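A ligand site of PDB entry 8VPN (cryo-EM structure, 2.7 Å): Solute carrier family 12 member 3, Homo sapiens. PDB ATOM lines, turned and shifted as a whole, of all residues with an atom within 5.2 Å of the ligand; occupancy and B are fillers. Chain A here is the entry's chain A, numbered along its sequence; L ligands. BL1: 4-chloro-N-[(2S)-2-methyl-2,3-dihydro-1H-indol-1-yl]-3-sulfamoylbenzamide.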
ATOM      1  N   ASN A 148     -15.837  10.214 -23.382  1.00  0.00           N
ATOM      2  CA  ASN A 148     -16.211  10.889 -22.134  1.00  0.00           C
ATOM      3  C   ASN A 148     -17.413  11.798 -22.325  1.00  0.00           C
ATOM      4  O   ASN A 148     -18.223  11.961 -21.401  1.00  0.00           O
ATOM      5  CB  ASN A 148     -15.022  11.681 -21.596  1.00  0.00           C
ATOM      6  CG  ASN A 148     -15.053  11.813 -20.091  1.00  0.00           C
ATOM      7  OD1 ASN A 148     -14.097  12.298 -19.483  1.00  0.00           O
ATOM      8  ND2 ASN A 148     -16.148  11.390 -19.478  1.00  0.00           N
ATOM      9  N   PHE A 222     -10.074  18.516  -7.800  1.00  0.00           N
ATOM     10  CA  PHE A 222     -10.224  17.831  -9.077  1.00  0.00           C
ATOM     11  C   PHE A 222     -10.081  16.317  -8.911  1.00  0.00           C
ATOM     12  O   PHE A 222     -10.884  15.536  -9.455  1.00  0.00           O
ATOM     13  CB  PHE A 222      -9.176  18.362 -10.059  1.00  0.00           C
ATOM     14  CG  PHE A 222      -9.569  18.262 -11.496  1.00  0.00           C
ATOM     15  CD1 PHE A 222     -10.477  19.136 -12.053  1.00  0.00           C
ATOM     16  CD2 PHE A 222      -9.015  17.275 -12.302  1.00  0.00           C
ATOM     17  CE1 PHE A 222     -10.844  19.027 -13.371  1.00  0.00           C
ATOM     18  CE2 PHE A 222      -9.374  17.172 -13.624  1.00  0.00           C
ATOM     19  CZ  PHE A 222     -10.285  18.058 -14.164  1.00  0.00           C
ATOM     20  N   ASN A 226     -13.066  13.444  -9.679  1.00  0.00           N
ATOM     21  CA  ASN A 226     -12.949  12.297 -10.582  1.00  0.00           C
ATOM     22  C   ASN A 226     -13.185  10.987  -9.837  1.00  0.00           C
ATOM     23  O   ASN A 226     -13.882  10.082 -10.342  1.00  0.00           O
ATOM     24  CB  ASN A 226     -11.572  12.295 -11.255  1.00  0.00           C
ATOM     25  CG  ASN A 226     -11.543  13.144 -12.502  1.00  0.00           C
ATOM     26  OD1 ASN A 226     -11.760  12.653 -13.604  1.00  0.00           O
ATOM     27  ND2 ASN A 226     -11.250  14.429 -12.338  1.00  0.00           N
ATOM     28  N   GLY A 229     -16.871  10.614  -9.567  1.00  0.00           N
ATOM     29  CA  GLY A 229     -17.540  10.386 -10.831  1.00  0.00           C
ATOM     30  C   GLY A 229     -17.453   8.941 -11.275  1.00  0.00           C
ATOM     31  O   GLY A 229     -18.390   8.423 -11.906  1.00  0.00           O
ATOM     32  N   MET A 232     -20.271   7.232  -9.605  1.00  0.00           N
ATOM     33  CA  MET A 232     -21.541   7.630 -10.194  1.00  0.00           C
ATOM     34  C   MET A 232     -21.838   6.829 -11.466  1.00  0.00           C
ATOM     35  O   MET A 232     -22.908   6.227 -11.615  1.00  0.00           O
ATOM     36  CB  MET A 232     -21.536   9.131 -10.498  1.00  0.00           C
ATOM     37  CG  MET A 232     -21.630  10.015  -9.271  1.00  0.00           C
ATOM     38  SD  MET A 232     -21.591  11.763  -9.685  1.00  0.00           S
ATOM     39  CE  MET A 232     -22.087  12.499  -8.134  1.00  0.00           C
ATOM     40  N   HIS A 233     -20.875   6.806 -12.397  1.00  0.00           N
ATOM     41  CA  HIS A 233     -21.091   6.094 -13.655  1.00  0.00           C
ATOM     42  C   HIS A 233     -21.309   4.604 -13.417  1.00  0.00           C
ATOM     43  O   HIS A 233     -22.158   3.981 -14.085  1.00  0.00           O
ATOM     44  CB  HIS A 233     -19.902   6.335 -14.592  1.00  0.00           C
ATOM     45  CG  HIS A 233     -19.742   7.760 -15.014  1.00  0.00           C
ATOM     46  ND1 HIS A 233     -18.599   8.489 -14.755  1.00  0.00           N
ATOM     47  CD2 HIS A 233     -20.566   8.584 -15.705  1.00  0.00           C
ATOM     48  CE1 HIS A 233     -18.734   9.706 -15.257  1.00  0.00           C
ATOM     49  NE2 HIS A 233     -19.924   9.789 -15.830  1.00  0.00           N
ATOM     50  N   PRO A 348     -25.194  19.262 -18.201  1.00  0.00           N
ATOM     51  CA  PRO A 348     -24.094  18.427 -17.700  1.00  0.00           C
ATOM     52  C   PRO A 348     -23.717  17.297 -18.634  1.00  0.00           C
ATOM     53  O   PRO A 348     -22.639  16.702 -18.465  1.00  0.00           O
ATOM     54  CB  PRO A 348     -24.627  17.895 -16.356  1.00  0.00           C
ATOM     55  CG  PRO A 348     -25.779  18.755 -16.010  1.00  0.00           C
ATOM     56  CD  PRO A 348     -26.357  19.232 -17.303  1.00  0.00           C
ATOM     57  N   SER A 349     -24.565  16.967 -19.604  1.00  0.00           N
ATOM     58  CA  SER A 349     -24.308  15.789 -20.428  1.00  0.00           C
ATOM     59  C   SER A 349     -23.066  15.932 -21.303  1.00  0.00           C
ATOM     60  O   SER A 349     -22.495  14.922 -21.704  1.00  0.00           O
ATOM     61  CB  SER A 349     -25.519  15.492 -21.311  1.00  0.00           C
ATOM     62  OG  SER A 349     -25.118  14.898 -22.523  1.00  0.00           O
ATOM     63  N   THR A 351     -19.663  17.837 -20.819  1.00  0.00           N
ATOM     64  CA  THR A 351     -18.628  18.637 -20.202  1.00  0.00           C
ATOM     65  C   THR A 351     -17.316  17.876 -19.970  1.00  0.00           C
ATOM     66  O   THR A 351     -16.385  18.472 -19.428  1.00  0.00           O
ATOM     67  CB  THR A 351     -19.104  19.218 -18.860  1.00  0.00           C
ATOM     68  OG1 THR A 351     -19.305  18.151 -17.919  1.00  0.00           O
ATOM     69  CG2 THR A 351     -20.401  19.983 -19.044  1.00  0.00           C
ATOM     70  N   GLY A 352     -17.228  16.614 -20.367  1.00  0.00           N
ATOM     71  CA  GLY A 352     -16.015  15.850 -20.149  1.00  0.00           C
ATOM     72  C   GLY A 352     -15.016  15.979 -21.283  1.00  0.00           C
ATOM     73  O   GLY A 352     -14.838  15.045 -22.064  1.00  0.00           O
ATOM     74  N   ILE A 353     -14.361  17.131 -21.385  1.00  0.00           N
ATOM     75  CA  ILE A 353     -13.485  17.445 -22.505  1.00  0.00           C
ATOM     76  C   ILE A 353     -12.019  17.393 -22.137  1.00  0.00           C
ATOM     77  O   ILE A 353     -11.157  17.560 -23.016  1.00  0.00           O
ATOM     78  CB  ILE A 353     -13.833  18.813 -23.116  1.00  0.00           C
ATOM     79  CG1 ILE A 353     -13.280  19.944 -22.251  1.00  0.00           C
ATOM     80  CG2 ILE A 353     -15.332  18.957 -23.271  1.00  0.00           C
ATOM     81  CD1 ILE A 353     -13.032  21.215 -23.017  1.00  0.00           C
ATOM     82  N   LEU A 354     -11.690  17.166 -20.868  1.00  0.00           N
ATOM     83  CA  LEU A 354     -10.310  17.055 -20.427  1.00  0.00           C
ATOM     84  C   LEU A 354      -9.865  15.612 -20.246  1.00  0.00           C
ATOM     85  O   LEU A 354      -8.814  15.361 -19.656  1.00  0.00           O
ATOM     86  CB  LEU A 354     -10.103  17.816 -19.119  1.00  0.00           C
ATOM     87  CG  LEU A 354     -10.605  19.255 -19.040  1.00  0.00           C
ATOM     88  CD1 LEU A 354     -10.408  19.782 -17.638  1.00  0.00           C
ATOM     89  CD2 LEU A 354      -9.881  20.143 -20.044  1.00  0.00           C
ATOM     90  N   ALA A 355     -10.647  14.651 -20.740  1.00  0.00           N
ATOM     91  CA  ALA A 355     -10.306  13.243 -20.539  1.00  0.00           C
ATOM     92  C   ALA A 355      -9.023  12.851 -21.246  1.00  0.00           C
ATOM     93  O   ALA A 355      -8.376  11.872 -20.844  1.00  0.00           O
ATOM     94  CB  ALA A 355     -11.456  12.353 -21.018  1.00  0.00           C
ATOM     95  N   ASN A 358      -5.537  14.744 -19.481  1.00  0.00           N
ATOM     96  CA  ASN A 358      -5.123  14.242 -18.174  1.00  0.00           C
ATOM     97  C   ASN A 358      -4.033  13.181 -18.276  1.00  0.00           C
ATOM     98  O   ASN A 358      -3.286  12.982 -17.309  1.00  0.00           O
ATOM     99  CB  ASN A 358      -6.332  13.694 -17.425  1.00  0.00           C
ATOM    100  CG  ASN A 358      -7.154  14.790 -16.783  1.00  0.00           C
ATOM    101  OD1 ASN A 358      -8.192  14.525 -16.169  1.00  0.00           O
ATOM    102  ND2 ASN A 358      -6.706  16.027 -16.913  1.00  0.00           N
ATOM    103  N   ALA A 470     -12.414   6.319 -17.828  1.00  0.00           N
ATOM    104  CA  ALA A 470     -11.729   7.585 -18.024  1.00  0.00           C
ATOM    105  C   ALA A 470     -11.573   8.332 -16.702  1.00  0.00           C
ATOM    106  O   ALA A 470     -10.479   8.826 -16.381  1.00  0.00           O
ATOM    107  CB  ALA A 470     -12.496   8.450 -19.036  1.00  0.00           C
ATOM    108  N   CYS A 471     -12.647   8.390 -15.909  1.00  0.00           N
ATOM    109  CA  CYS A 471     -12.569   9.094 -14.632  1.00  0.00           C
ATOM    110  C   CYS A 471     -11.510   8.465 -13.730  1.00  0.00           C
ATOM    111  O   CYS A 471     -10.693   9.180 -13.116  1.00  0.00           O
ATOM    112  CB  CYS A 471     -13.926   9.097 -13.945  1.00  0.00           C
ATOM    113  SG  CYS A 471     -15.085  10.321 -14.592  1.00  0.00           S
ATOM    114  N   SER A 474      -7.858   9.293 -14.936  1.00  0.00           N
ATOM    115  CA  SER A 474      -7.537  10.700 -14.752  1.00  0.00           C
ATOM    116  C   SER A 474      -7.255  11.009 -13.289  1.00  0.00           C
ATOM    117  O   SER A 474      -6.285  11.704 -12.952  1.00  0.00           O
ATOM    118  CB  SER A 474      -8.693  11.562 -15.268  1.00  0.00           C
ATOM    119  OG  SER A 474      -9.012  11.225 -16.609  1.00  0.00           O
ATOM    120  N   ILE A 531     -20.266  17.707  -7.080  1.00  0.00           N
ATOM    121  CA  ILE A 531     -19.261  17.317  -8.064  1.00  0.00           C
ATOM    122  C   ILE A 531     -19.354  18.183  -9.306  1.00  0.00           C
ATOM    123  O   ILE A 531     -18.339  18.631  -9.863  1.00  0.00           O
ATOM    124  CB  ILE A 531     -19.421  15.823  -8.407  1.00  0.00           C
ATOM    125  CG1 ILE A 531     -19.641  15.001  -7.135  1.00  0.00           C
ATOM    126  CG2 ILE A 531     -18.219  15.302  -9.175  1.00  0.00           C
ATOM    127  CD1 ILE A 531     -18.842  15.461  -5.943  1.00  0.00           C
ATOM    128  N   SER A 532     -20.584  18.423  -9.784  1.00  0.00           N
ATOM    129  CA  SER A 532     -20.750  19.278 -10.959  1.00  0.00           C
ATOM    130  C   SER A 532     -20.150  20.655 -10.721  1.00  0.00           C
ATOM    131  O   SER A 532     -19.420  21.192 -11.564  1.00  0.00           O
ATOM    132  CB  SER A 532     -22.226  19.394 -11.322  1.00  0.00           C
ATOM    133  OG  SER A 532     -22.812  18.114 -11.488  1.00  0.00           O
ATOM    134  N   PHE A 535     -16.393  20.699 -10.895  1.00  0.00           N
ATOM    135  CA  PHE A 535     -15.907  20.721 -12.272  1.00  0.00           C
ATOM    136  C   PHE A 535     -16.041  22.110 -12.887  1.00  0.00           C
ATOM    137  O   PHE A 535     -15.140  22.581 -13.610  1.00  0.00           O
ATOM    138  CB  PHE A 535     -16.660  19.691 -13.115  1.00  0.00           C
ATOM    139  CG  PHE A 535     -16.233  18.273 -12.857  1.00  0.00           C
ATOM    140  CD1 PHE A 535     -14.943  17.857 -13.148  1.00  0.00           C
ATOM    141  CD2 PHE A 535     -17.124  17.347 -12.350  1.00  0.00           C
ATOM    142  CE1 PHE A 535     -14.553  16.566 -12.919  1.00  0.00           C
ATOM    143  CE2 PHE A 535     -16.733  16.039 -12.123  1.00  0.00           C
ATOM    144  CZ  PHE A 535     -15.451  15.651 -12.409  1.00  0.00           C
ATOM    145  N   TYR A 539     -13.275  24.697 -14.640  1.00  0.00           N
ATOM    146  CA  TYR A 539     -13.423  25.468 -15.876  1.00  0.00           C
ATOM    147  C   TYR A 539     -13.059  26.940 -15.655  1.00  0.00           C
ATOM    148  O   TYR A 539     -12.297  27.545 -16.442  1.00  0.00           O
ATOM    149  CB  TYR A 539     -14.856  25.394 -16.397  1.00  0.00           C
ATOM    150  CG  TYR A 539     -15.191  24.198 -17.269  1.00  0.00           C
ATOM    151  CD1 TYR A 539     -14.531  22.990 -17.112  1.00  0.00           C
ATOM    152  CD2 TYR A 539     -16.153  24.297 -18.264  1.00  0.00           C
ATOM    153  CE1 TYR A 539     -14.838  21.908 -17.909  1.00  0.00           C
ATOM    154  CE2 TYR A 539     -16.467  23.221 -19.066  1.00  0.00           C
ATOM    155  CZ  TYR A 539     -15.802  22.036 -18.888  1.00  0.00           C
ATOM    156  OH  TYR A 539     -16.118  20.965 -19.682  1.00  0.00           O
HETATM  157  OAW BL1 L   1     -12.819  15.012 -18.146  1.00  0.00           O
HETATM  158  SAX BL1 L   1     -13.066  14.742 -16.833  1.00  0.00           S
HETATM  159  NAS BL1 L   1     -12.820  13.113 -16.549  1.00  0.00           N
HETATM  160  OAV BL1 L   1     -12.067  15.441 -16.179  1.00  0.00           O
HETATM  161  CAO BL1 L   1     -14.687  15.329 -16.527  1.00  0.00           C
HETATM  162  CAM BL1 L   1     -15.674  14.423 -16.255  1.00  0.00           C
HETATM  163  CAJ BL1 L   1     -15.034  16.662 -16.558  1.00  0.00           C
HETATM  164 CLAQ BL1 L   1     -13.860  17.953 -16.886  1.00  0.00          CL
HETATM  165  CAC BL1 L   1     -16.321  17.057 -16.338  1.00  0.00           C
HETATM  166  CAN BL1 L   1     -17.278  16.141 -16.079  1.00  0.00           C
HETATM  167  CAL BL1 L   1     -16.954  14.836 -16.045  1.00  0.00           C
HETATM  168  CAK BL1 L   1     -17.931  13.797 -15.757  1.00  0.00           C
HETATM  169  OAU BL1 L   1     -17.687  12.716 -16.199  1.00  0.00           O
HETATM  170  NAR BL1 L   1     -19.040  14.072 -14.931  1.00  0.00           N
HETATM  171  NAT BL1 L   1     -19.905  13.015 -14.673  1.00  0.00           N
HETATM  172  CAI BL1 L   1     -20.309  12.799 -13.264  1.00  0.00           C
HETATM  173  CAP BL1 L   1     -20.211  14.105 -12.515  1.00  0.00           C
HETATM  174  CAA BL1 L   1     -21.124  12.986 -15.419  1.00  0.00           C
HETATM  175  CAB BL1 L   1     -22.185  12.548 -14.683  1.00  0.00           C
HETATM  176  CAF BL1 L   1     -21.735  12.271 -13.289  1.00  0.00           C
HETATM  177  CAD BL1 L   1     -21.348  13.288 -16.745  1.00  0.00           C
HETATM  178  CAH BL1 L   1     -22.612  13.164 -17.290  1.00  0.00           C
HETATM  179  CAG BL1 L   1     -23.656  12.721 -16.523  1.00  0.00           C
HETATM  180  CAE BL1 L   1     -23.446  12.406 -15.191  1.00  0.00           C
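NE2 of His 233 lies close to NAT of the ligand (3.4 Å).
Residues that only touch the ligand: Thr 351 (3.4 Å), Phe 535 (3.6 Å), Met 232 (3.6 Å), Leu 354 (3.7 Å), Pro 348 (3.7 Å), Phe 222 (3.8 Å), Gly 352 (3.8 Å), Cys 471 (3.9 Å) and Asn 358 (3.98 Å).
Of the 21 residues printed, 13 come within 4 Å of the ligand.
The side-chain amide nitrogen of Asn 226 is in hydrogen-bond range of the backbone carbonyl oxygen of Phe 222.
The backbone carbonyl oxygen (O) of Gly 229 lies within hydrogen-bond range of a ring nitrogen (ND1) of His 233, at 2.9 Å.
The backbone carbonyl oxygen of Thr 351 sits at hydrogen-bond distance from the side-chain hydroxyl of Tyr 539 (2.5 Å).
The side-chain amide oxygen (OD1) of Asn 358 lies close to the side-chain hydroxyl (OG) of Ser 474, at 3.4 Å.
The side-chain amide oxygen (OD1) of Asn 226 sits at hydrogen-bond distance from a nitrogen (NAS) of the ligand.
The side-chain amide oxygen of Asn 148 lies close to an oxygen (OAW) of the ligand.
N of Ala 355 is in hydrogen-bond range of OAW of the ligand (3.4 Å).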
